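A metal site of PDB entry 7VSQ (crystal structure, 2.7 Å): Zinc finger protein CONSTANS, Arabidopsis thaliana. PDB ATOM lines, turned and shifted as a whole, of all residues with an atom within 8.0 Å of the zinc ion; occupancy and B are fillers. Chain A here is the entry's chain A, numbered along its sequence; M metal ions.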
ATOM      1  N   PRO A  11      13.957  -3.034   7.663  1.00  0.00           N
ATOM      2  CA  PRO A  11      14.742  -1.978   8.272  1.00  0.00           C
ATOM      3  C   PRO A  11      15.964  -2.587   8.943  1.00  0.00           C
ATOM      4  O   PRO A  11      15.994  -3.783   9.234  1.00  0.00           O
ATOM      5  CB  PRO A  11      13.774  -1.394   9.288  1.00  0.00           C
ATOM      6  CG  PRO A  11      12.948  -2.598   9.736  1.00  0.00           C
ATOM      7  CD  PRO A  11      12.988  -3.618   8.605  1.00  0.00           C
ATOM      8  N   CYS A  12      16.966  -1.765   9.180  1.00  0.00           N
ATOM      9  CA  CYS A  12      18.224  -2.243   9.720  1.00  0.00           C
ATOM     10  C   CYS A  12      17.996  -2.616  11.190  1.00  0.00           C
ATOM     11  O   CYS A  12      17.351  -1.877  11.921  1.00  0.00           O
ATOM     12  CB  CYS A  12      19.303  -1.185   9.556  1.00  0.00           C
ATOM     13  SG  CYS A  12      20.799  -1.491  10.468  1.00  0.00           S
ATOM     14  N   ASP A  13      18.444  -3.788  11.610  1.00  0.00           N
ATOM     15  CA  ASP A  13      18.178  -4.217  12.985  1.00  0.00           C
ATOM     16  C   ASP A  13      18.967  -3.549  14.131  1.00  0.00           C
ATOM     17  O   ASP A  13      18.483  -3.579  15.267  1.00  0.00           O
ATOM     18  CB  ASP A  13      18.342  -5.737  13.090  1.00  0.00           C
ATOM     19  CG  ASP A  13      17.425  -6.479  12.132  1.00  0.00           C
ATOM     20  OD1 ASP A  13      16.226  -6.113  12.043  1.00  0.00           O
ATOM     21  OD2 ASP A  13      17.891  -7.443  11.491  1.00  0.00           O
ATOM     22  N   THR A  14      20.134  -2.952  13.898  1.00  0.00           N
ATOM     23  CA  THR A  14      20.750  -2.211  15.006  1.00  0.00           C
ATOM     24  C   THR A  14      20.097  -0.844  15.114  1.00  0.00           C
ATOM     25  O   THR A  14      19.615  -0.469  16.176  1.00  0.00           O
ATOM     26  CB  THR A  14      22.276  -2.037  14.848  1.00  0.00           C
ATOM     27  OG1 THR A  14      22.876  -3.279  14.466  1.00  0.00           O
ATOM     28  CG2 THR A  14      22.898  -1.594  16.164  1.00  0.00           C
ATOM     29  N   CYS A  15      20.113  -0.090  14.031  1.00  0.00           N
ATOM     30  CA  CYS A  15      19.346   1.154  13.984  1.00  0.00           C
ATOM     31  C   CYS A  15      18.173   0.859  13.062  1.00  0.00           C
ATOM     32  O   CYS A  15      18.362   0.562  11.887  1.00  0.00           O
ATOM     33  CB  CYS A  15      20.188   2.348  13.524  1.00  0.00           C
ATOM     34  SG  CYS A  15      20.535   2.500  11.751  1.00  0.00           S
ATOM     35  N   ARG A  16      16.953   0.939  13.594  1.00  0.00           N
ATOM     36  CA  ARG A  16      15.772   0.545  12.836  1.00  0.00           C
ATOM     37  C   ARG A  16      15.402   1.594  11.794  1.00  0.00           C
ATOM     38  O   ARG A  16      14.439   1.439  11.040  1.00  0.00           O
ATOM     39  CB  ARG A  16      14.603   0.254  13.798  1.00  0.00           C
ATOM     40  CG  ARG A  16      14.994  -0.732  14.883  1.00  0.00           C
ATOM     41  CD  ARG A  16      13.827  -1.538  15.419  1.00  0.00           C
ATOM     42  NE  ARG A  16      13.970  -2.970  15.130  1.00  0.00           N
ATOM     43  CZ  ARG A  16      14.683  -3.819  15.882  1.00  0.00           C
ATOM     44  NH1 ARG A  16      15.318  -3.382  16.957  1.00  0.00           N
ATOM     45  NH2 ARG A  16      14.766  -5.094  15.551  1.00  0.00           N
ATOM     46  N   SER A  17      16.208   2.662  11.751  1.00  0.00           N
ATOM     47  CA  SER A  17      16.035   3.794  10.835  1.00  0.00           C
ATOM     48  C   SER A  17      16.452   3.637   9.363  1.00  0.00           C
ATOM     49  O   SER A  17      15.801   4.185   8.466  1.00  0.00           O
ATOM     50  CB  SER A  17      16.830   4.968  11.413  1.00  0.00           C
ATOM     51  OG  SER A  17      17.539   5.636  10.374  1.00  0.00           O
ATOM     52  N   ASN A  18      17.494   2.864   9.091  1.00  0.00           N
ATOM     53  CA  ASN A  18      17.912   2.648   7.707  1.00  0.00           C
ATOM     54  C   ASN A  18      17.420   1.302   7.241  1.00  0.00           C
ATOM     55  O   ASN A  18      16.753   0.577   7.984  1.00  0.00           O
ATOM     56  CB  ASN A  18      19.434   2.732   7.569  1.00  0.00           C
ATOM     57  CG  ASN A  18      19.950   4.152   7.738  1.00  0.00           C
ATOM     58  OD1 ASN A  18      19.184   5.067   8.019  1.00  0.00           O
ATOM     59  ND2 ASN A  18      21.261   4.334   7.591  1.00  0.00           N
ATOM     60  N   ALA A  19      17.800   0.938   6.027  1.00  0.00           N
ATOM     61  CA  ALA A  19      17.328  -0.308   5.455  1.00  0.00           C
ATOM     62  C   ALA A  19      18.542  -1.189   5.434  1.00  0.00           C
ATOM     63  O   ALA A  19      19.668  -0.695   5.399  1.00  0.00           O
ATOM     64  CB  ALA A  19      16.752  -0.109   4.070  1.00  0.00           C
ATOM     65  N   CYS A  20      18.331  -2.492   5.443  1.00  0.00           N
ATOM     66  CA  CYS A  20      19.457  -3.379   5.573  1.00  0.00           C
ATOM     67  C   CYS A  20      20.123  -3.580   4.228  1.00  0.00           C
ATOM     68  O   CYS A  20      19.462  -3.582   3.195  1.00  0.00           O
ATOM     69  CB  CYS A  20      19.020  -4.724   6.158  1.00  0.00           C
ATOM     70  SG  CYS A  20      17.835  -5.605   5.141  1.00  0.00           S
ATOM     71  N   THR A  21      21.432  -3.743   4.252  1.00  0.00           N
ATOM     72  CA  THR A  21      22.202  -3.900   3.030  1.00  0.00           C
ATOM     73  C   THR A  21      22.946  -5.221   3.101  1.00  0.00           C
ATOM     74  O   THR A  21      23.261  -5.823   2.074  1.00  0.00           O
ATOM     75  CB  THR A  21      23.182  -2.737   2.808  1.00  0.00           C
ATOM     76  OG1 THR A  21      24.236  -2.789   3.771  1.00  0.00           O
ATOM     77  CG2 THR A  21      22.450  -1.395   2.856  1.00  0.00           C
ATOM     78  N   TYR A  30      20.054  -8.551  10.064  1.00  0.00           N
ATOM     79  CA  TYR A  30      20.233  -7.838   8.820  1.00  0.00           C
ATOM     80  C   TYR A  30      20.553  -6.362   9.110  1.00  0.00           C
ATOM     81  O   TYR A  30      19.815  -5.720   9.841  1.00  0.00           O
ATOM     82  CB  TYR A  30      18.976  -7.973   7.954  1.00  0.00           C
ATOM     83  CG  TYR A  30      18.648  -9.416   7.602  1.00  0.00           C
ATOM     84  CD1 TYR A  30      18.914  -9.941   6.344  1.00  0.00           C
ATOM     85  CD2 TYR A  30      18.066 -10.260   8.547  1.00  0.00           C
ATOM     86  CE1 TYR A  30      18.610 -11.268   6.041  1.00  0.00           C
ATOM     87  CE2 TYR A  30      17.771 -11.563   8.255  1.00  0.00           C
ATOM     88  CZ  TYR A  30      18.050 -12.071   7.004  1.00  0.00           C
ATOM     89  OH  TYR A  30      17.746 -13.379   6.712  1.00  0.00           O
ATOM     90  N   LEU A  31      21.629  -5.852   8.538  1.00  0.00           N
ATOM     91  CA  LEU A  31      22.075  -4.506   8.885  1.00  0.00           C
ATOM     92  C   LEU A  31      22.216  -3.575   7.678  1.00  0.00           C
ATOM     93  O   LEU A  31      22.273  -4.020   6.536  1.00  0.00           O
ATOM     94  CB  LEU A  31      23.410  -4.584   9.616  1.00  0.00           C
ATOM     95  CG  LEU A  31      23.255  -5.140  11.033  1.00  0.00           C
ATOM     96  CD1 LEU A  31      24.580  -5.180  11.779  1.00  0.00           C
ATOM     97  CD2 LEU A  31      22.198  -4.374  11.800  1.00  0.00           C
ATOM     98  N   CYS A  32      22.310  -2.286   7.964  1.00  0.00           N
ATOM     99  CA  CYS A  32      22.745  -1.295   6.978  1.00  0.00           C
ATOM    100  C   CYS A  32      24.273  -1.295   7.082  1.00  0.00           C
ATOM    101  O   CYS A  32      24.832  -1.983   7.928  1.00  0.00           O
ATOM    102  CB  CYS A  32      22.191   0.103   7.241  1.00  0.00           C
ATOM    103  SG  CYS A  32      22.855   0.868   8.714  1.00  0.00           S
ATOM    104  N   MET A  33      24.939  -0.533   6.227  1.00  0.00           N
ATOM    105  CA  MET A  33      26.390  -0.525   6.216  1.00  0.00           C
ATOM    106  C   MET A  33      27.133   0.220   7.340  1.00  0.00           C
ATOM    107  O   MET A  33      28.243  -0.169   7.720  1.00  0.00           O
ATOM    108  CB  MET A  33      26.867   0.020   4.869  1.00  0.00           C
ATOM    109  CG  MET A  33      28.367  -0.036   4.678  1.00  0.00           C
ATOM    110  SD  MET A  33      28.887   0.489   3.044  1.00  0.00           S
ATOM    111  CE  MET A  33      28.025  -0.717   2.028  1.00  0.00           C
ATOM    112  N   SER A  34      26.507   1.218   7.964  1.00  0.00           N
ATOM    113  CA  SER A  34      27.203   1.961   9.006  1.00  0.00           C
ATOM    114  C   SER A  34      27.097   1.167  10.296  1.00  0.00           C
ATOM    115  O   SER A  34      28.030   1.159  11.121  1.00  0.00           O
ATOM    116  CB  SER A  34      26.613   3.361   9.172  1.00  0.00           C
ATOM    117  OG  SER A  34      27.584   4.278   9.651  1.00  0.00           O
ATOM    118  N   CYS A  35      25.998   0.454  10.444  1.00  0.00           N
ATOM    119  CA  CYS A  35      25.838  -0.428  11.577  1.00  0.00           C
ATOM    120  C   CYS A  35      26.804  -1.580  11.347  1.00  0.00           C
ATOM    121  O   CYS A  35      27.533  -1.947  12.253  1.00  0.00           O
ATOM    122  CB  CYS A  35      24.393  -0.894  11.749  1.00  0.00           C
ATOM    123  SG  CYS A  35      23.273   0.515  11.923  1.00  0.00           S
ATOM    124  N   ASP A  36      26.778  -2.160  10.154  1.00  0.00           N
ATOM    125  CA  ASP A  36      27.672  -3.271   9.840  1.00  0.00           C
ATOM    126  C   ASP A  36      29.113  -2.966  10.237  1.00  0.00           C
ATOM    127  O   ASP A  36      29.757  -3.738  10.951  1.00  0.00           O
ATOM    128  CB  ASP A  36      27.619  -3.597   8.357  1.00  0.00           C
ATOM    129  CG  ASP A  36      28.538  -4.730   7.984  1.00  0.00           C
ATOM    130  OD1 ASP A  36      28.213  -5.876   8.341  1.00  0.00           O
ATOM    131  OD2 ASP A  36      29.600  -4.469   7.376  1.00  0.00           O
ATOM    132  N   GLN A  38      30.180  -0.548  12.225  1.00  0.00           N
ATOM    133  CA  GLN A  38      30.277  -0.257  13.659  1.00  0.00           C
ATOM    134  C   GLN A  38      30.373  -1.513  14.516  1.00  0.00           C
ATOM    135  O   GLN A  38      31.285  -1.663  15.325  1.00  0.00           O
ATOM    136  CB  GLN A  38      29.066   0.567  14.112  1.00  0.00           C
ATOM    137  CG  GLN A  38      28.795   0.500  15.613  1.00  0.00           C
ATOM    138  CD  GLN A  38      27.317   0.384  15.924  1.00  0.00           C
ATOM    139  OE1 GLN A  38      26.460   0.713  15.093  1.00  0.00           O
ATOM    140  NE2 GLN A  38      27.003  -0.084  17.121  1.00  0.00           N
HETATM  141 ZN    ZN M   1      21.435   0.661  10.462  1.00  0.00          ZN
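SG of Cys 12 lies close to N of Thr 14 (3.8 Å). The backbone NH (N) of Cys 12 lies within hydrogen-bond range of the backbone carbonyl oxygen (O) of Asn 18, 2.6 Å away. SG of Cys 32 lies close to N of Ser 34.
SG of Cys 12 is bound to the zinc ion, at 2.2 Å. SG of Cys 32 is bound to the zinc ion (2.3 Å). The zinc ion is bound by SG of Cys 35, at 2.4 Å. The zinc ion is bound by SG of Cys 15 (2.4 Å).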
